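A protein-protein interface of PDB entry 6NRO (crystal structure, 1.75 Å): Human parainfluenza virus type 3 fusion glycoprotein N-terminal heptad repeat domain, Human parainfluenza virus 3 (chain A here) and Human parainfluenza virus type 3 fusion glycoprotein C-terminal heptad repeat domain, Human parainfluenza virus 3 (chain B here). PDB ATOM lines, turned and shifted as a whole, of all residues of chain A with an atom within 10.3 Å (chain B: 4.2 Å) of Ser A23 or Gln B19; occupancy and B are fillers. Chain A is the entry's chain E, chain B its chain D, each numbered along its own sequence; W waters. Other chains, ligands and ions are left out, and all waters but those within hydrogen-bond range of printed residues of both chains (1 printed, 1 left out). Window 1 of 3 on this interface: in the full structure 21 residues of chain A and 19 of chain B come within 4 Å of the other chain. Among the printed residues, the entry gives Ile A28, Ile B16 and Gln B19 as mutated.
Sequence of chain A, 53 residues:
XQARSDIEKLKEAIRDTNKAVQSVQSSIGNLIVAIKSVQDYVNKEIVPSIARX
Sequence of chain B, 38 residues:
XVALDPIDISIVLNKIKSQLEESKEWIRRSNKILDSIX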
ATOM      1  N   ARG A  15     -30.611  35.336  -7.048  1.00  0.00           N
ATOM      2  CA  ARG A  15     -29.578  36.045  -7.836  1.00  0.00           C
ATOM      3  C   ARG A  15     -28.213  35.436  -7.510  1.00  0.00           C
ATOM      4  O   ARG A  15     -27.464  35.237  -8.422  1.00  0.00           O
ATOM      5  CB  ARG A  15     -29.698  37.562  -7.679  1.00  0.00           C
ATOM      6  CG  ARG A  15     -30.771  38.135  -8.596  1.00  0.00           C
ATOM      7  CD  ARG A  15     -30.567  39.555  -9.069  1.00  0.00           C
ATOM      8  NE  ARG A  15     -30.174  40.433  -7.989  1.00  0.00           N
ATOM      9  CZ  ARG A  15     -30.924  41.408  -7.503  1.00  0.00           C
ATOM     10  NH1 ARG A  15     -31.564  42.217  -8.328  1.00  0.00           N
ATOM     11  NH2 ARG A  15     -31.019  41.574  -6.195  1.00  0.00           N
ATOM     12  N   ASP A  16     -27.945  35.099  -6.262  1.00  0.00           N
ATOM     13  CA  ASP A  16     -26.660  34.486  -5.867  1.00  0.00           C
ATOM     14  C   ASP A  16     -26.592  33.090  -6.486  1.00  0.00           C
ATOM     15  O   ASP A  16     -25.557  32.713  -7.001  1.00  0.00           O
ATOM     16  CB  ASP A  16     -26.506  34.474  -4.356  1.00  0.00           C
ATOM     17  CG  ASP A  16     -26.263  35.863  -3.819  1.00  0.00           C
ATOM     18  OD1 ASP A  16     -26.344  36.043  -2.620  1.00  0.00           O
ATOM     19  OD2 ASP A  16     -26.007  36.723  -4.625  1.00  0.00           O
ATOM     20  N   THR A  17     -27.684  32.352  -6.460  1.00  0.00           N
ATOM     21  CA  THR A  17     -27.689  31.020  -7.046  1.00  0.00           C
ATOM     22  C   THR A  17     -27.377  31.069  -8.538  1.00  0.00           C
ATOM     23  O   THR A  17     -26.642  30.224  -9.055  1.00  0.00           O
ATOM     24  CB  THR A  17     -29.035  30.356  -6.793  1.00  0.00           C
ATOM     25  OG1 THR A  17     -29.233  30.220  -5.382  1.00  0.00           O
ATOM     26  CG2 THR A  17     -29.103  28.992  -7.454  1.00  0.00           C
ATOM     27  N   ASN A  18     -27.913  32.055  -9.250  1.00  0.00           N
ATOM     28  CA  ASN A  18     -27.600  32.164 -10.670  1.00  0.00           C
ATOM     29  C   ASN A  18     -26.122  32.476 -10.880  1.00  0.00           C
ATOM     30  O   ASN A  18     -25.489  31.948 -11.801  1.00  0.00           O
ATOM     31  CB  ASN A  18     -28.497  33.227 -11.310  1.00  0.00           C
ATOM     32  CG  ASN A  18     -29.968  32.781 -11.394  1.00  0.00           C
ATOM     33  OD1 ASN A  18     -30.275  31.593 -11.289  1.00  0.00           O
ATOM     34  ND2 ASN A  18     -30.865  33.735 -11.598  1.00  0.00           N
ATOM     35  N   LYS A  19     -25.554  33.335 -10.037  1.00  0.00           N
ATOM     36  CA  LYS A  19     -24.128  33.607 -10.137  1.00  0.00           C
ATOM     37  C   LYS A  19     -23.329  32.336  -9.883  1.00  0.00           C
ATOM     38  O   LYS A  19     -22.311  32.085 -10.545  1.00  0.00           O
ATOM     39  CB  LYS A  19     -23.745  34.713  -9.153  1.00  0.00           C
ATOM     40  CG  LYS A  19     -24.316  36.089  -9.526  1.00  0.00           C
ATOM     41  CD  LYS A  19     -23.944  37.144  -8.496  1.00  0.00           C
ATOM     42  CE  LYS A  19     -24.269  38.556  -8.993  1.00  0.00           C
ATOM     43  NZ  LYS A  19     -25.446  39.160  -8.329  1.00  0.00           N
ATOM     44  N   ALA A  20     -23.791  31.512  -8.946  1.00  0.00           N
ATOM     45  CA  ALA A  20     -23.109  30.256  -8.692  1.00  0.00           C
ATOM     46  C   ALA A  20     -23.203  29.349  -9.907  1.00  0.00           C
ATOM     47  O   ALA A  20     -22.263  28.607 -10.204  1.00  0.00           O
ATOM     48  CB  ALA A  20     -23.682  29.557  -7.459  1.00  0.00           C
ATOM     49  N   VAL A  21     -24.326  29.376 -10.619  1.00  0.00           N
ATOM     50  CA  VAL A  21     -24.405  28.555 -11.819  1.00  0.00           C
ATOM     51  C   VAL A  21     -23.501  29.121 -12.903  1.00  0.00           C
ATOM     52  O   VAL A  21     -22.891  28.372 -13.679  1.00  0.00           O
ATOM     53  CB  VAL A  21     -25.867  28.452 -12.284  1.00  0.00           C
ATOM     54  CG1 VAL A  21     -25.966  27.734 -13.601  1.00  0.00           C
ATOM     55  CG2 VAL A  21     -26.690  27.737 -11.217  1.00  0.00           C
ATOM     56  N   GLN A  22     -23.426  30.453 -12.990  1.00  0.00           N
ATOM     57  CA  GLN A  22     -22.585  31.098 -13.988  1.00  0.00           C
ATOM     58  C   GLN A  22     -21.125  30.736 -13.781  1.00  0.00           C
ATOM     59  O   GLN A  22     -20.397  30.507 -14.749  1.00  0.00           O
ATOM     60  CB  GLN A  22     -22.798  32.616 -13.944  1.00  0.00           C
ATOM     61  CG  GLN A  22     -24.161  33.047 -14.503  1.00  0.00           C
ATOM     62  CD  GLN A  22     -24.376  34.558 -14.523  1.00  0.00           C
ATOM     63  OE1 GLN A  22     -23.947  35.295 -13.630  1.00  0.00           O
ATOM     64  NE2 GLN A  22     -25.046  35.024 -15.565  1.00  0.00           N
ATOM     65  N   SER A  23     -20.676  30.637 -12.527  1.00  0.00           N
ATOM     66  CA  SER A  23     -19.310  30.167 -12.292  1.00  0.00           C
ATOM     67  C   SER A  23     -19.156  28.712 -12.714  1.00  0.00           C
ATOM     68  O   SER A  23     -18.131  28.320 -13.290  1.00  0.00           O
ATOM     69  CB  SER A  23     -18.933  30.343 -10.816  1.00  0.00           C
ATOM     70  OG  SER A  23     -18.782  31.710 -10.454  1.00  0.00           O
ATOM     71  N   VAL A  24     -20.168  27.889 -12.447  1.00  0.00           N
ATOM     72  CA  VAL A  24     -20.096  26.495 -12.877  1.00  0.00           C
ATOM     73  C   VAL A  24     -19.996  26.414 -14.391  1.00  0.00           C
ATOM     74  O   VAL A  24     -19.226  25.611 -14.939  1.00  0.00           O
ATOM     75  CB  VAL A  24     -21.300  25.713 -12.331  1.00  0.00           C
ATOM     76  CG1 VAL A  24     -21.540  24.481 -13.174  1.00  0.00           C
ATOM     77  CG2 VAL A  24     -20.990  25.346 -10.888  1.00  0.00           C
ATOM     78  N   GLN A  25     -20.750  27.265 -15.089  1.00  0.00           N
ATOM     79  CA  GLN A  25     -20.685  27.295 -16.542  1.00  0.00           C
ATOM     80  C   GLN A  25     -19.278  27.627 -17.007  1.00  0.00           C
ATOM     81  O   GLN A  25     -18.764  26.995 -17.931  1.00  0.00           O
ATOM     82  CB  GLN A  25     -21.700  28.297 -17.091  1.00  0.00           C
ATOM     83  CG  GLN A  25     -23.158  27.854 -16.864  1.00  0.00           C
ATOM     84  CD  GLN A  25     -24.169  28.961 -17.032  1.00  0.00           C
ATOM     85  OE1 GLN A  25     -23.856  30.143 -16.877  1.00  0.00           O
ATOM     86  NE2 GLN A  25     -25.401  28.582 -17.354  1.00  0.00           N
ATOM     87  N   SER A  26     -18.631  28.596 -16.375  1.00  0.00           N
ATOM     88  CA  SER A  26     -17.240  28.984 -16.710  1.00  0.00           C
ATOM     89  C   SER A  26     -16.332  27.765 -16.538  1.00  0.00           C
ATOM     90  O   SER A  26     -15.546  27.489 -17.404  1.00  0.00           O
ATOM     91  CB  SER A  26     -16.790  30.111 -15.862  1.00  0.00           C
ATOM     92  OG  SER A  26     -17.636  31.221 -16.033  1.00  0.00           O
ATOM     93  N   SER A  27     -16.469  27.073 -15.419  1.00  0.00           N
ATOM     94  CA  SER A  27     -15.706  25.859 -15.071  1.00  0.00           C
ATOM     95  C   SER A  27     -15.825  24.824 -16.180  1.00  0.00           C
ATOM     96  O   SER A  27     -14.831  24.270 -16.566  1.00  0.00           O
ATOM     97  CB  SER A  27     -16.206  25.276 -13.808  1.00  0.00           C
ATOM     98  OG  SER A  27     -15.654  25.966 -12.733  1.00  0.00           O
ATOM     99  N   ILE A  28     -17.030  24.592 -16.665  1.00  0.00           N
ATOM    100  CA  ILE A  28     -17.266  23.558 -17.704  1.00  0.00           C
ATOM    101  C   ILE A  28     -16.591  24.002 -18.996  1.00  0.00           C
ATOM    102  O   ILE A  28     -16.021  23.172 -19.664  1.00  0.00           O
ATOM    103  CB  ILE A  28     -18.760  23.256 -17.840  1.00  0.00           C
ATOM    104  CG1 ILE A  28     -19.226  22.436 -16.636  1.00  0.00           C
ATOM    105  CG2 ILE A  28     -19.059  22.559 -19.146  1.00  0.00           C
ATOM    106  CD1 ILE A  28     -20.679  22.528 -16.383  1.00  0.00           C
ATOM    107  N   GLY A  29     -16.638  25.291 -19.282  1.00  0.00           N
ATOM    108  CA  GLY A  29     -15.980  25.849 -20.463  1.00  0.00           C
ATOM    109  C   GLY A  29     -14.514  25.501 -20.429  1.00  0.00           C
ATOM    110  O   GLY A  29     -14.009  25.113 -21.450  1.00  0.00           O
ATOM    111  N   ASN A  30     -13.874  25.623 -19.268  1.00  0.00           N
ATOM    112  CA  ASN A  30     -12.450  25.346 -19.121  1.00  0.00           C
ATOM    113  C   ASN A  30     -12.175  23.856 -19.073  1.00  0.00           C
ATOM    114  O   ASN A  30     -11.098  23.415 -19.494  1.00  0.00           O
ATOM    115  CB  ASN A  30     -11.900  26.011 -17.860  1.00  0.00           C
ATOM    116  CG  ASN A  30     -11.684  27.482 -18.043  1.00  0.00           C
ATOM    117  OD1 ASN A  30     -11.212  27.909 -19.091  1.00  0.00           O
ATOM    118  ND2 ASN A  30     -12.064  28.278 -17.044  1.00  0.00           N
ATOM    119  N   LEU A  31     -13.107  23.067 -18.533  1.00  0.00           N
ATOM    120  CA  LEU A  31     -12.965  21.619 -18.601  1.00  0.00           C
ATOM    121  C   LEU A  31     -12.940  21.138 -20.047  1.00  0.00           C
ATOM    122  O   LEU A  31     -12.265  20.158 -20.364  1.00  0.00           O
ATOM    123  CB  LEU A  31     -14.103  20.938 -17.838  1.00  0.00           C
ATOM    124  CG  LEU A  31     -13.950  20.860 -16.319  1.00  0.00           C
ATOM    125  CD1 LEU A  31     -15.239  20.366 -15.673  1.00  0.00           C
ATOM    126  CD2 LEU A  31     -12.795  19.955 -15.911  1.00  0.00           C
ATOM    127  N   ILE A  32     -13.697  21.781 -20.928  1.00  0.00           N
ATOM    128  CA  ILE A  32     -13.595  21.458 -22.348  1.00  0.00           C
ATOM    129  C   ILE A  32     -12.193  21.770 -22.848  1.00  0.00           C
ATOM    130  O   ILE A  32     -11.567  20.978 -23.565  1.00  0.00           O
ATOM    131  CB  ILE A  32     -14.654  22.239 -23.146  1.00  0.00           C
ATOM    132  CG1 ILE A  32     -16.061  21.838 -22.722  1.00  0.00           C
ATOM    133  CG2 ILE A  32     -14.454  22.061 -24.624  1.00  0.00           C
ATOM    134  CD1 ILE A  32     -17.131  22.704 -23.331  1.00  0.00           C
ATOM    135  N   VAL A  33     -11.676  22.938 -22.471  1.00  0.00           N
ATOM    136  CA  VAL A  33     -10.349  23.322 -22.944  1.00  0.00           C
ATOM    137  C   VAL A  33      -9.307  22.332 -22.451  1.00  0.00           C
ATOM    138  O   VAL A  33      -8.430  21.912 -23.208  1.00  0.00           O
ATOM    139  CB  VAL A  33     -10.004  24.758 -22.508  1.00  0.00           C
ATOM    140  CG1 VAL A  33      -8.475  25.083 -22.794  1.00  0.00           C
ATOM    141  CG2 VAL A  33     -10.916  25.746 -23.170  1.00  0.00           C
ATOM    142  N   LYS B  15      -7.478  27.201 -12.755  1.00  0.00           N
ATOM    143  CA  LYS B  15      -8.543  28.163 -13.094  1.00  0.00           C
ATOM    144  C   LYS B  15      -9.892  27.557 -12.696  1.00  0.00           C
ATOM    145  O   LYS B  15     -10.677  28.242 -12.084  1.00  0.00           O
ATOM    146  CB  LYS B  15      -8.485  28.496 -14.581  1.00  0.00           C
ATOM    147  CG  LYS B  15      -9.431  29.589 -15.029  1.00  0.00           C
ATOM    148  CD  LYS B  15      -8.873  30.431 -16.139  1.00  0.00           C
ATOM    149  CE  LYS B  15      -8.685  29.680 -17.434  1.00  0.00           C
ATOM    150  NZ  LYS B  15      -7.701  30.345 -18.315  1.00  0.00           N
ATOM    151  N   ILE B  16     -10.137  26.296 -13.023  1.00  0.00           N
ATOM    152  CA  ILE B  16     -11.408  25.659 -12.683  1.00  0.00           C
ATOM    153  C   ILE B  16     -11.576  25.573 -11.170  1.00  0.00           C
ATOM    154  O   ILE B  16     -12.667  25.826 -10.641  1.00  0.00           O
ATOM    155  CB  ILE B  16     -11.516  24.277 -13.347  1.00  0.00           C
ATOM    156  CG1 ILE B  16     -11.421  24.429 -14.865  1.00  0.00           C
ATOM    157  CG2 ILE B  16     -12.812  23.574 -12.909  1.00  0.00           C
ATOM    158  CD1 ILE B  16     -11.020  23.163 -15.588  1.00  0.00           C
ATOM    159  N   LYS B  17     -10.510  25.217 -10.461  1.00  0.00           N
ATOM    160  CA  LYS B  17     -10.546  25.117  -8.984  1.00  0.00           C
ATOM    161  C   LYS B  17     -10.962  26.471  -8.429  1.00  0.00           C
ATOM    162  O   LYS B  17     -11.757  26.509  -7.513  1.00  0.00           O
ATOM    163  CB  LYS B  17      -9.195  24.701  -8.400  1.00  0.00           C
ATOM    164  CG  LYS B  17      -8.793  23.262  -8.650  1.00  0.00           C
ATOM    165  CD  LYS B  17      -7.515  22.874  -7.959  1.00  0.00           C
ATOM    166  CE  LYS B  17      -6.405  22.495  -8.911  1.00  0.00           C
ATOM    167  NZ  LYS B  17      -5.071  22.765  -8.338  1.00  0.00           N
ATOM    168  N   SER B  18     -10.431  27.543  -8.991  1.00  0.00           N
ATOM    169  CA  SER B  18     -10.686  28.929  -8.544  1.00  0.00           C
ATOM    170  C   SER B  18     -12.151  29.289  -8.790  1.00  0.00           C
ATOM    171  O   SER B  18     -12.754  29.871  -7.929  1.00  0.00           O
ATOM    172  CB  SER B  18      -9.761  29.872  -9.222  1.00  0.00           C
ATOM    173  OG  SER B  18     -10.254  31.184  -9.148  1.00  0.00           O
ATOM    174  N   GLN B  19     -12.709  28.910  -9.928  1.00  0.00           N
ATOM    175  CA  GLN B  19     -14.113  29.231 -10.271  1.00  0.00           C
ATOM    176  C   GLN B  19     -15.065  28.408  -9.404  1.00  0.00           C
ATOM    177  O   GLN B  19     -16.161  28.877  -9.140  1.00  0.00           O
ATOM    178  CB  GLN B  19     -14.331  29.013 -11.756  1.00  0.00           C
ATOM    179  CG  GLN B  19     -13.378  29.843 -12.574  1.00  0.00           C
ATOM    180  CD  GLN B  19     -13.525  29.538 -14.029  1.00  0.00           C
ATOM    181  OE1 GLN B  19     -13.746  28.409 -14.412  1.00  0.00           O
ATOM    182  NE2 GLN B  19     -13.420  30.557 -14.845  1.00  0.00           N
ATOM    183  N   LEU B  20     -14.648  27.214  -9.008  1.00  0.00           N
ATOM    184  CA  LEU B  20     -15.443  26.309  -8.155  1.00  0.00           C
ATOM    185  C   LEU B  20     -15.598  26.950  -6.769  1.00  0.00           C
ATOM    186  O   LEU B  20     -16.695  26.951  -6.248  1.00  0.00           O
ATOM    187  CB  LEU B  20     -14.720  24.972  -8.096  1.00  0.00           C
ATOM    188  CG  LEU B  20     -15.630  23.765  -8.012  1.00  0.00           C
ATOM    189  CD1 LEU B  20     -16.621  23.764  -9.153  1.00  0.00           C
ATOM    190  CD2 LEU B  20     -14.816  22.493  -8.001  1.00  0.00           C
ATOM    191  N   GLU B  21     -14.516  27.490  -6.221  1.00  0.00           N
ATOM    192  CA  GLU B  21     -14.493  28.173  -4.907  1.00  0.00           C
ATOM    193  C   GLU B  21     -15.452  29.351  -4.957  1.00  0.00           C
ATOM    194  O   GLU B  21     -16.146  29.569  -3.988  1.00  0.00           O
ATOM    195  CB  GLU B  21     -13.094  28.674  -4.569  1.00  0.00           C
ATOM    196  CG  GLU B  21     -12.168  27.564  -4.163  1.00  0.00           C
ATOM    197  CD  GLU B  21     -12.707  26.757  -3.011  1.00  0.00           C
ATOM    198  OE1 GLU B  21     -12.795  25.546  -3.136  1.00  0.00           O
ATOM    199  OE2 GLU B  21     -13.053  27.369  -2.008  1.00  0.00           O
ATOM    200  N   GLU B  22     -15.471  30.079  -6.056  1.00  0.00           N
ATOM    201  CA  GLU B  22     -16.380  31.235  -6.233  1.00  0.00           C
ATOM    202  C   GLU B  22     -17.817  30.707  -6.188  1.00  0.00           C
ATOM    203  O   GLU B  22     -18.611  31.230  -5.426  1.00  0.00           O
ATOM    204  CB  GLU B  22     -16.128  31.948  -7.551  1.00  0.00           C
ATOM    205  CG  GLU B  22     -14.791  32.627  -7.619  1.00  0.00           C
ATOM    206  CD  GLU B  22     -14.741  33.729  -8.655  1.00  0.00           C
ATOM    207  OE1 GLU B  22     -15.478  33.657  -9.618  1.00  0.00           O
ATOM    208  OE2 GLU B  22     -13.973  34.660  -8.472  1.00  0.00           O
ATOM    209  N   SER B  23     -18.102  29.678  -6.972  1.00  0.00           N
ATOM    210  CA  SER B  23     -19.441  29.057  -7.074  1.00  0.00           C
ATOM    211  C   SER B  23     -19.916  28.675  -5.675  1.00  0.00           C
ATOM    212  O   SER B  23     -21.047  28.961  -5.346  1.00  0.00           O
ATOM    213  CB  SER B  23     -19.422  27.881  -7.993  1.00  0.00           C
ATOM    214  OG  SER B  23     -20.715  27.365  -8.166  1.00  0.00           O
HETATM  215  O   HOH W   1     -12.552  31.297 -17.458  1.00  0.00           O
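Ser A23 touches Gln B19 (CB to O, 3.6 Å). Ser A23 touches Glu B22 (OG to OE1, 3.9 Å). Ser B23 touches Ser A23 (CB to CB, 3.8 Å). Val A24 touches Ser B23. C of Ser A26 touches OE1 of Gln B19, 3.4 Å away. OG of Ser A27 touches O of Ile B16 (3.6 Å). Lys B15 touches Asn A30. Ile B16 touches Asn A30 (CG1 to CB, 3.4 Å). CD1 of Ile B16 touches N of Leu A31, 3.6 Å away.
Hydrophobic or aromatic side chains of chain B within 4 Å of the printed part of chain A: Ile B16. Among the printed residues, no Asp or Glu carboxylate lies within 4 Å of a Lys or Arg side-chain nitrogen of the other chain.
Water W1 lies within hydrogen-bond range of the side-chain amide nitrogen of Gln B19 and the side-chain amide nitrogen of Asn A30.
The backbone carbonyl oxygen of Ala A20 sits at hydrogen-bond distance from the side-chain hydroxyl of Ser B23 (2.8 Å). The side-chain amide oxygen of Gln B19 sits at hydrogen-bond distance from the backbone NH of Ser A27. The side-chain amide nitrogen of Asn A30 sits at hydrogen-bond distance from the side-chain amide oxygen of Gln B19 (3.1 Å).
Of chain B, only Gln B19 (3.6 Å), Glu B22 (3.9 Å) and Ser B23 (3.8 Å) come within 4 Å of Ser A23. Of chain A, only Ser A23, Ser A26, Ser A27 and Asn A30 come within 4 Å of Gln B19. Ile B16 touches just these residues of chain A: Ser A27 (3.6 Å), Asn A30 (3.4 Å) and Leu A31 (3.6 Å). No residue of chain A comes within 4 Å of Leu B20. Glu B22 touches just one residue of chain A: Ser A23. Printed residues of chain A within 4 Å of Lys B15: Asn A30. Printed residues of chain B within 4 Å of Leu A31: Ile B16 (3.6 Å). Of the printed residues of chain B, Val A24 touches Ser B23 (3.4 Å). Of the printed residues of chain B, Ser A26 touches Gln B19 (3.4 Å). Printed residues of chain B within 4 Å of Asn A30: Lys B15 (3.5 Å), Ile B16 (3.4 Å) and Gln B19 (3.1 Å). Lys B17 touches none of the printed residues of chain A. The nearest printed residue of chain B that does not touch Ser A23 is Leu B20 (5.6 Å).
The backbone carbonyl oxygen of Gln A22 sits at hydrogen-bond distance from the side-chain hydroxyl of Ser A26 (3.1 Å). O of Ser A23 sits at hydrogen-bond distance from OG of Ser A27 (3.5 Å).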
